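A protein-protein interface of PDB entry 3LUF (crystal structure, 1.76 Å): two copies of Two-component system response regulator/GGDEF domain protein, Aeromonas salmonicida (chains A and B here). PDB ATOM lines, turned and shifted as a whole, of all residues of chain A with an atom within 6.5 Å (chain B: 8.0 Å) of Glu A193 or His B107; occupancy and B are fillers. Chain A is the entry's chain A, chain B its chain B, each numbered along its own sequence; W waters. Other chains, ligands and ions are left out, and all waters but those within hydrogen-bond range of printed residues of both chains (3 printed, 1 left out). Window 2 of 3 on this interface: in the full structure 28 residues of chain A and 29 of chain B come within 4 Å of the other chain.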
ATOM      1  N   VAL A 188     -27.801   9.570  11.442  1.00  0.00           N
ATOM      2  CA  VAL A 188     -27.228  10.889  11.501  1.00  0.00           C
ATOM      3  C   VAL A 188     -27.600  11.676  10.243  1.00  0.00           C
ATOM      4  O   VAL A 188     -27.974  12.848  10.334  1.00  0.00           O
ATOM      5  CB  VAL A 188     -25.729  10.832  11.668  1.00  0.00           C
ATOM      6  CG1 VAL A 188     -25.097  12.257  11.538  1.00  0.00           C
ATOM      7  CG2 VAL A 188     -25.412  10.147  13.040  1.00  0.00           C
ATOM      8  N   ARG A 189     -27.473  11.040   9.084  1.00  0.00           N
ATOM      9  CA  ARG A 189     -27.893  11.691   7.836  1.00  0.00           C
ATOM     10  C   ARG A 189     -29.353  12.145   7.905  1.00  0.00           C
ATOM     11  O   ARG A 189     -29.660  13.305   7.612  1.00  0.00           O
ATOM     12  CB  ARG A 189     -27.639  10.789   6.643  1.00  0.00           C
ATOM     13  CG  ARG A 189     -26.210  10.344   6.546  1.00  0.00           C
ATOM     14  CD  ARG A 189     -25.928   9.627   5.244  1.00  0.00           C
ATOM     15  NE  ARG A 189     -26.468  10.353   4.099  1.00  0.00           N
ATOM     16  CZ  ARG A 189     -25.733  10.842   3.105  1.00  0.00           C
ATOM     17  NH1 ARG A 189     -24.411  10.688   3.110  1.00  0.00           N
ATOM     18  NH2 ARG A 189     -26.326  11.490   2.106  1.00  0.00           N
ATOM     19  N   MET A 190     -30.248  11.264   8.351  1.00  0.00           N
ATOM     20  CA  MET A 190     -31.666  11.639   8.436  1.00  0.00           C
ATOM     21  C   MET A 190     -31.890  12.815   9.352  1.00  0.00           C
ATOM     22  O   MET A 190     -32.621  13.769   9.021  1.00  0.00           O
ATOM     23  CB  MET A 190     -32.526  10.443   8.916  1.00  0.00           C
ATOM     24  CG  MET A 190     -32.662   9.393   7.821  1.00  0.00           C
ATOM     25  SD  MET A 190     -33.831   7.935   8.418  1.00  0.00           S
ATOM     26  CE  MET A 190     -35.492   8.886   8.294  1.00  0.00           C
ATOM     27  N   LEU A 191     -31.217  12.782  10.502  1.00  0.00           N
ATOM     28  CA  LEU A 191     -31.410  13.843  11.468  1.00  0.00           C
ATOM     29  C   LEU A 191     -30.851  15.157  10.952  1.00  0.00           C
ATOM     30  O   LEU A 191     -31.442  16.188  11.148  1.00  0.00           O
ATOM     31  CB  LEU A 191     -30.792  13.491  12.823  1.00  0.00           C
ATOM     32  CG  LEU A 191     -31.466  12.300  13.527  1.00  0.00           C
ATOM     33  CD1 LEU A 191     -30.652  11.960  14.782  1.00  0.00           C
ATOM     34  CD2 LEU A 191     -32.916  12.643  13.799  1.00  0.00           C
ATOM     35  N   ARG A 192     -29.711  15.103  10.290  1.00  0.00           N
ATOM     36  CA  ARG A 192     -29.096  16.341   9.775  1.00  0.00           C
ATOM     37  C   ARG A 192     -29.801  16.941   8.564  1.00  0.00           C
ATOM     38  O   ARG A 192     -29.606  18.149   8.255  1.00  0.00           O
ATOM     39  CB  ARG A 192     -27.591  16.109   9.501  1.00  0.00           C
ATOM     40  CG  ARG A 192     -26.753  16.098  10.795  1.00  0.00           C
ATOM     41  CD  ARG A 192     -26.614  17.498  11.370  1.00  0.00           C
ATOM     42  NE  ARG A 192     -25.931  17.414  12.664  1.00  0.00           N
ATOM     43  CZ  ARG A 192     -26.531  17.527  13.840  1.00  0.00           C
ATOM     44  NH1 ARG A 192     -27.843  17.800  13.925  1.00  0.00           N
ATOM     45  NH2 ARG A 192     -25.794  17.345  14.939  1.00  0.00           N
ATOM     46  N   GLU A 193     -30.643  16.139   7.891  1.00  0.00           N
ATOM     47  CA  GLU A 193     -31.506  16.669   6.848  1.00  0.00           C
ATOM     48  C   GLU A 193     -32.559  17.651   7.384  1.00  0.00           C
ATOM     49  O   GLU A 193     -33.038  18.502   6.637  1.00  0.00           O
ATOM     50  CB  GLU A 193     -32.142  15.527   6.026  1.00  0.00           C
ATOM     51  CG  GLU A 193     -31.118  14.861   5.082  1.00  0.00           C
ATOM     52  CD  GLU A 193     -31.773  13.893   4.116  1.00  0.00           C
ATOM     53  OE1 GLU A 193     -32.683  13.196   4.546  1.00  0.00           O
ATOM     54  OE2 GLU A 193     -31.375  13.847   2.933  1.00  0.00           O
ATOM     55  N   ARG A 194     -32.860  17.554   8.683  1.00  0.00           N
ATOM     56  CA  ARG A 194     -33.877  18.342   9.352  1.00  0.00           C
ATOM     57  C   ARG A 194     -33.315  19.322  10.359  1.00  0.00           C
ATOM     58  O   ARG A 194     -33.865  20.411  10.510  1.00  0.00           O
ATOM     59  CB  ARG A 194     -34.852  17.429  10.109  1.00  0.00           C
ATOM     60  CG  ARG A 194     -35.674  16.565   9.200  1.00  0.00           C
ATOM     61  CD  ARG A 194     -36.770  15.810   9.992  1.00  0.00           C
ATOM     62  NE  ARG A 194     -37.889  16.672  10.387  1.00  0.00           N
ATOM     63  CZ  ARG A 194     -38.829  16.325  11.275  1.00  0.00           C
ATOM     64  NH1 ARG A 194     -38.782  15.144  11.895  1.00  0.00           N
ATOM     65  NH2 ARG A 194     -39.830  17.164  11.553  1.00  0.00           N
ATOM     66  N   TYR A 195     -32.234  18.929  11.053  1.00  0.00           N
ATOM     67  CA  TYR A 195     -31.783  19.653  12.251  1.00  0.00           C
ATOM     68  C   TYR A 195     -30.302  20.004  12.225  1.00  0.00           C
ATOM     69  O   TYR A 195     -29.458  19.144  11.912  1.00  0.00           O
ATOM     70  CB  TYR A 195     -32.035  18.794  13.491  1.00  0.00           C
ATOM     71  CG  TYR A 195     -33.470  18.410  13.639  1.00  0.00           C
ATOM     72  CD1 TYR A 195     -34.467  19.411  13.669  1.00  0.00           C
ATOM     73  CD2 TYR A 195     -33.855  17.074  13.673  1.00  0.00           C
ATOM     74  CE1 TYR A 195     -35.826  19.086  13.761  1.00  0.00           C
ATOM     75  CE2 TYR A 195     -35.233  16.732  13.793  1.00  0.00           C
ATOM     76  CZ  TYR A 195     -36.192  17.756  13.822  1.00  0.00           C
ATOM     77  OH  TYR A 195     -37.536  17.465  13.925  1.00  0.00           O
ATOM     78  N   LYS A 197     -26.570  21.277  13.962  1.00  0.00           N
ATOM     79  CA  LYS A 197     -25.760  20.941  15.157  1.00  0.00           C
ATOM     80  C   LYS A 197     -26.106  21.751  16.399  1.00  0.00           C
ATOM     81  O   LYS A 197     -25.734  21.375  17.513  1.00  0.00           O
ATOM     82  CB  LYS A 197     -24.280  21.153  14.886  1.00  0.00           C
ATOM     83  CG  LYS A 197     -23.596  20.102  14.074  1.00  0.00           C
ATOM     84  CD  LYS A 197     -22.089  20.328  14.152  1.00  0.00           C
ATOM     85  CE  LYS A 197     -21.461  20.263  12.793  1.00  0.00           C
ATOM     86  NZ  LYS A 197     -22.062  21.268  11.869  1.00  0.00           N
ATOM     87  N   LYS A 219     -18.131  13.819   9.215  1.00  0.00           N
ATOM     88  CA  LYS A 219     -18.375  14.349   7.891  1.00  0.00           C
ATOM     89  C   LYS A 219     -19.861  14.384   7.546  1.00  0.00           C
ATOM     90  O   LYS A 219     -20.227  15.150   6.696  1.00  0.00           O
ATOM     91  CB  LYS A 219     -17.500  13.654   6.848  1.00  0.00           C
ATOM     92  CG  LYS A 219     -15.997  14.099   7.077  1.00  0.00           C
ATOM     93  CD  LYS A 219     -15.098  13.566   6.038  1.00  0.00           C
ATOM     94  CE  LYS A 219     -13.596  13.698   6.372  1.00  0.00           C
ATOM     95  NZ  LYS A 219     -13.213  14.973   6.919  1.00  0.00           N
ATOM     96  N   GLN A 220     -20.685  13.591   8.248  1.00  0.00           N
ATOM     97  CA  GLN A 220     -22.154  13.627   8.084  1.00  0.00           C
ATOM     98  C   GLN A 220     -22.844  14.596   9.041  1.00  0.00           C
ATOM     99  O   GLN A 220     -24.081  14.790   8.993  1.00  0.00           O
ATOM    100  CB  GLN A 220     -22.761  12.220   8.197  1.00  0.00           C
ATOM    101  CG  GLN A 220     -22.503  11.392   6.934  1.00  0.00           C
ATOM    102  CD  GLN A 220     -23.002  12.075   5.669  1.00  0.00           C
ATOM    103  OE1 GLN A 220     -22.215  12.311   4.737  1.00  0.00           O
ATOM    104  NE2 GLN A 220     -24.307  12.411   5.629  1.00  0.00           N
ATOM    105  N   GLY A 221     -22.043  15.239   9.894  1.00  0.00           N
ATOM    106  CA  GLY A 221     -22.567  16.319  10.725  1.00  0.00           C
ATOM    107  C   GLY A 221     -22.723  15.978  12.213  1.00  0.00           C
ATOM    108  O   GLY A 221     -23.295  16.777  12.973  1.00  0.00           O
ATOM    109  N   MET B  19     -23.719  27.072  -2.777  1.00  0.00           N
ATOM    110  CA  MET B  19     -23.943  26.679  -1.356  1.00  0.00           C
ATOM    111  C   MET B  19     -22.736  26.965  -0.479  1.00  0.00           C
ATOM    112  O   MET B  19     -22.869  27.477   0.656  1.00  0.00           O
ATOM    113  CB  MET B  19     -24.264  25.192  -1.234  1.00  0.00           C
ATOM    114  CG  MET B  19     -25.641  24.854  -1.661  1.00  0.00           C
ATOM    115  SD  MET B  19     -25.830  22.875  -1.655  1.00  0.00           S
ATOM    116  CE  MET B  19     -27.731  23.049  -1.833  1.00  0.00           C
ATOM    117  N   VAL B 101     -14.066  16.801   2.210  1.00  0.00           N
ATOM    118  CA  VAL B 101     -15.417  17.201   2.577  1.00  0.00           C
ATOM    119  C   VAL B 101     -16.355  16.418   1.690  1.00  0.00           C
ATOM    120  O   VAL B 101     -16.168  16.364   0.469  1.00  0.00           O
ATOM    121  CB  VAL B 101     -15.639  18.718   2.354  1.00  0.00           C
ATOM    122  CG1 VAL B 101     -17.096  19.123   2.591  1.00  0.00           C
ATOM    123  CG2 VAL B 101     -14.747  19.512   3.294  1.00  0.00           C
ATOM    124  N   MET B 102     -17.342  15.764   2.296  1.00  0.00           N
ATOM    125  CA  MET B 102     -18.375  15.125   1.486  1.00  0.00           C
ATOM    126  C   MET B 102     -19.324  16.168   0.918  1.00  0.00           C
ATOM    127  O   MET B 102     -19.751  17.078   1.656  1.00  0.00           O
ATOM    128  CB  MET B 102     -19.165  14.117   2.334  1.00  0.00           C
ATOM    129  CG  MET B 102     -18.331  12.994   2.905  1.00  0.00           C
ATOM    130  SD  MET B 102     -17.441  11.855   1.565  1.00  0.00           S
ATOM    131  CE  MET B 102     -18.871  11.400   0.371  1.00  0.00           C
ATOM    132  N   LYS B 103     -19.659  16.053  -0.375  1.00  0.00           N
ATOM    133  CA  LYS B 103     -20.572  17.021  -0.998  1.00  0.00           C
ATOM    134  C   LYS B 103     -21.842  16.389  -1.542  1.00  0.00           C
ATOM    135  O   LYS B 103     -22.435  16.904  -2.488  1.00  0.00           O
ATOM    136  CB  LYS B 103     -19.879  17.913  -2.050  1.00  0.00           C
ATOM    137  CG  LYS B 103     -19.184  17.135  -3.141  1.00  0.00           C
ATOM    138  CD  LYS B 103     -18.797  18.041  -4.297  1.00  0.00           C
ATOM    139  CE  LYS B 103     -18.060  17.225  -5.378  1.00  0.00           C
ATOM    140  NZ  LYS B 103     -18.074  18.032  -6.646  1.00  0.00           N
ATOM    141  N   ASP B 104     -22.268  15.297  -0.905  1.00  0.00           N
ATOM    142  CA  ASP B 104     -23.462  14.578  -1.356  1.00  0.00           C
ATOM    143  C   ASP B 104     -24.758  15.173  -0.810  1.00  0.00           C
ATOM    144  O   ASP B 104     -25.818  14.821  -1.285  1.00  0.00           O
ATOM    145  CB  ASP B 104     -23.368  13.074  -1.054  1.00  0.00           C
ATOM    146  CG  ASP B 104     -23.264  12.777   0.431  1.00  0.00           C
ATOM    147  OD1 ASP B 104     -22.617  13.534   1.172  1.00  0.00           O
ATOM    148  OD2 ASP B 104     -23.833  11.750   0.857  1.00  0.00           O
ATOM    149  N   SER B 105     -24.660  16.105   0.130  1.00  0.00           N
ATOM    150  CA  SER B 105     -25.820  16.799   0.672  1.00  0.00           C
ATOM    151  C   SER B 105     -25.436  18.163   1.168  1.00  0.00           C
ATOM    152  O   SER B 105     -24.249  18.474   1.366  1.00  0.00           O
ATOM    153  CB  SER B 105     -26.460  16.027   1.844  1.00  0.00           C
ATOM    154  OG  SER B 105     -25.546  16.000   2.932  1.00  0.00           O
ATOM    155  N   ARG B 106     -26.445  18.978   1.420  1.00  0.00           N
ATOM    156  CA  ARG B 106     -26.201  20.305   1.944  1.00  0.00           C
ATOM    157  C   ARG B 106     -25.580  20.226   3.349  1.00  0.00           C
ATOM    158  O   ARG B 106     -24.608  20.941   3.662  1.00  0.00           O
ATOM    159  CB  ARG B 106     -27.489  21.134   1.951  1.00  0.00           C
ATOM    160  CG  ARG B 106     -27.327  22.502   2.631  1.00  0.00           C
ATOM    161  CD  ARG B 106     -26.170  23.371   2.055  1.00  0.00           C
ATOM    162  NE  ARG B 106     -26.016  24.594   2.857  1.00  0.00           N
ATOM    163  CZ  ARG B 106     -25.295  24.707   3.976  1.00  0.00           C
ATOM    164  NH1 ARG B 106     -24.588  23.681   4.462  1.00  0.00           N
ATOM    165  NH2 ARG B 106     -25.270  25.871   4.613  1.00  0.00           N
ATOM    166  N   HIS B 107     -26.095  19.314   4.176  1.00  0.00           N
ATOM    167  CA  HIS B 107     -25.586  19.161   5.543  1.00  0.00           C
ATOM    168  C   HIS B 107     -24.162  18.569   5.615  1.00  0.00           C
ATOM    169  O   HIS B 107     -23.418  18.852   6.544  1.00  0.00           O
ATOM    170  CB  HIS B 107     -26.581  18.370   6.442  1.00  0.00           C
ATOM    171  CG  HIS B 107     -26.590  16.892   6.174  1.00  0.00           C
ATOM    172  ND1 HIS B 107     -27.550  16.290   5.382  1.00  0.00           N
ATOM    173  CD2 HIS B 107     -25.750  15.901   6.564  1.00  0.00           C
ATOM    174  CE1 HIS B 107     -27.322  14.986   5.335  1.00  0.00           C
ATOM    175  NE2 HIS B 107     -26.221  14.729   6.021  1.00  0.00           N
ATOM    176  N   SER B 108     -23.765  17.769   4.629  1.00  0.00           N
ATOM    177  CA  SER B 108     -22.388  17.292   4.638  1.00  0.00           C
ATOM    178  C   SER B 108     -21.427  18.438   4.243  1.00  0.00           C
ATOM    179  O   SER B 108     -20.329  18.546   4.783  1.00  0.00           O
ATOM    180  CB  SER B 108     -22.214  16.018   3.821  1.00  0.00           C
ATOM    181  OG  SER B 108     -22.292  16.260   2.439  1.00  0.00           O
ATOM    182  N   LEU B 109     -21.863  19.300   3.333  1.00  0.00           N
ATOM    183  CA  LEU B 109     -21.060  20.488   2.963  1.00  0.00           C
ATOM    184  C   LEU B 109     -20.775  21.376   4.133  1.00  0.00           C
ATOM    185  O   LEU B 109     -19.743  22.034   4.175  1.00  0.00           O
ATOM    186  CB  LEU B 109     -21.788  21.331   1.898  1.00  0.00           C
ATOM    187  CG  LEU B 109     -21.679  20.895   0.476  1.00  0.00           C
ATOM    188  CD1 LEU B 109     -22.554  21.918  -0.331  1.00  0.00           C
ATOM    189  CD2 LEU B 109     -20.195  20.825  -0.044  1.00  0.00           C
ATOM    190  N   GLN B 110     -21.692  21.406   5.098  1.00  0.00           N
ATOM    191  CA  GLN B 110     -21.519  22.224   6.267  1.00  0.00           C
ATOM    192  C   GLN B 110     -20.192  21.910   6.980  1.00  0.00           C
ATOM    193  O   GLN B 110     -19.610  22.787   7.593  1.00  0.00           O
ATOM    194  CB  GLN B 110     -22.710  22.052   7.218  1.00  0.00           C
ATOM    195  CG  GLN B 110     -22.749  23.022   8.355  1.00  0.00           C
ATOM    196  CD  GLN B 110     -22.872  24.467   7.909  1.00  0.00           C
ATOM    197  OE1 GLN B 110     -23.369  24.772   6.816  1.00  0.00           O
ATOM    198  NE2 GLN B 110     -22.426  25.361   8.753  1.00  0.00           N
ATOM    199  N   TYR B 111     -19.721  20.664   6.902  1.00  0.00           N
ATOM    200  CA  TYR B 111     -18.411  20.317   7.472  1.00  0.00           C
ATOM    201  C   TYR B 111     -17.285  21.270   6.980  1.00  0.00           C
ATOM    202  O   TYR B 111     -16.399  21.671   7.753  1.00  0.00           O
ATOM    203  CB  TYR B 111     -18.048  18.855   7.165  1.00  0.00           C
ATOM    204  CG  TYR B 111     -16.727  18.396   7.726  1.00  0.00           C
ATOM    205  CD1 TYR B 111     -16.627  17.891   9.037  1.00  0.00           C
ATOM    206  CD2 TYR B 111     -15.571  18.460   6.956  1.00  0.00           C
ATOM    207  CE1 TYR B 111     -15.370  17.460   9.559  1.00  0.00           C
ATOM    208  CE2 TYR B 111     -14.349  18.046   7.455  1.00  0.00           C
ATOM    209  CZ  TYR B 111     -14.251  17.558   8.747  1.00  0.00           C
ATOM    210  OH  TYR B 111     -13.018  17.158   9.183  1.00  0.00           O
ATOM    211  N   ALA B 112     -17.325  21.611   5.701  1.00  0.00           N
ATOM    212  CA  ALA B 112     -16.281  22.470   5.108  1.00  0.00           C
ATOM    213  C   ALA B 112     -16.258  23.862   5.784  1.00  0.00           C
ATOM    214  O   ALA B 112     -15.201  24.498   5.954  1.00  0.00           O
ATOM    215  CB  ALA B 112     -16.529  22.572   3.598  1.00  0.00           C
HETATM  216  O   HOH W   1     -24.978  13.604   3.184  1.00  0.00           O
HETATM  217  O   HOH W   2     -13.822  14.227   9.763  1.00  0.00           O
HETATM  218  O   HOH W   3     -18.511  16.462   4.834  1.00  0.00           O
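The guanidinium group (NH1) of Arg A189 lies close to the side-chain amide nitrogen (NE2) of Gln A220 (3.1 Å).
The backbone carbonyl oxygen of Tyr A195 lies within hydrogen-bond range of the guanidinium group of Arg A192 (2.9 Å).
The backbone carbonyl oxygen of Met B102 sits at hydrogen-bond distance from the side-chain hydroxyl of Ser B108, at 2.8 Å.
The side-chain hydroxyl of Ser B108 is in hydrogen-bond range of the side-chain carboxylate of Asp B104 (3.0 Å).
A ring nitrogen (ND1) of His B107 sits close to the side-chain hydroxyl (OG) of Ser B105, at 3.2 Å.
The side-chain hydroxyl of Ser B105 sits at hydrogen-bond distance from the backbone NH of Ser B108.
No position is printed for both chains.
Of the 10 pairs that touch across the chains among the printed residues, none has its exchanged pair printed and touching as well.
NH1 of Arg A189 lies within salt-bridge range of OD2 of Asp B104, 2.6 Å away.
The side-chain hydroxyl (OH) of Tyr B111 sits at hydrogen-bond distance from the side-chain amino group (NZ) of Lys A219, 3.2 Å away.
The side-chain amide nitrogen (NE2) of Gln A220 sits at hydrogen-bond distance from a ring nitrogen (NE2) of His B107 (3.0 Å).
Among the printed residues, merely in contact across the chains: Arg A192 with His B107, Lys A219 with Ser B108, Arg A189 with His B107, Gln A220 with Asp B104, Glu A193 with His B107, Gln A220 with Ser B108 and Lys A197 with Gln B110.
Water W1 lies within hydrogen-bond range of the side-chain hydroxyl (OG) of Ser B105 (2.5 Å), the guanidinium group (NH2) of Arg A189 (2.7 Å), the side-chain amide nitrogen (NE2) of Gln A220 (2.8 Å), the side-chain carboxylate (OD1) of Asp B104 (3.1 Å) and a ring nitrogen (NE2) of His B107 (3.3 Å).
Water W3 lies within hydrogen-bond range of the backbone carbonyl oxygen of Ser B108, the backbone carbonyl oxygen of Lys A219 and the backbone NH of Met B102.
Water W2 bridges the side-chain amino group (NZ) of Lys A219 and the side-chain hydroxyl (OH) of Tyr B111.
Of the printed residues of chain B, Glu A193 touches His B107.
Of the printed residues of chain A, His B107 touches Arg A189, Arg A192, Glu A193 and Gln A220.
Printed residues of chain A within 4 Å of Ser B108: Lys A219 and Gln A220.
Of the printed residues of chain A, Tyr B111 touches Lys A219 (3.2 Å).
Printed residues of chain A within 4 Å of Asp B104: Arg A189 and Gln A220.
The nearest printed residue of chain B that does not touch Arg A189 is Ser B105 (4.5 Å).
Of the 13 printed residues of chain B, 5 touch a printed residue of chain A.
Printed residues of chain B that touch a printed residue of chain A: Asp B104, His B107, Ser B108, Gln B110 and Tyr B111.
Printed residues of chain A that touch a printed residue of chain B: Arg A189, Arg A192, Glu A193, Lys A197, Lys A219 and Gln A220.
Among the printed residues, 10 pairs touch across the chains.
Among the printed residues, Asp or Glu carboxylates within 4 Å of a Lys or Arg side-chain nitrogen of the other chain: Arg A189 with Asp B104.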
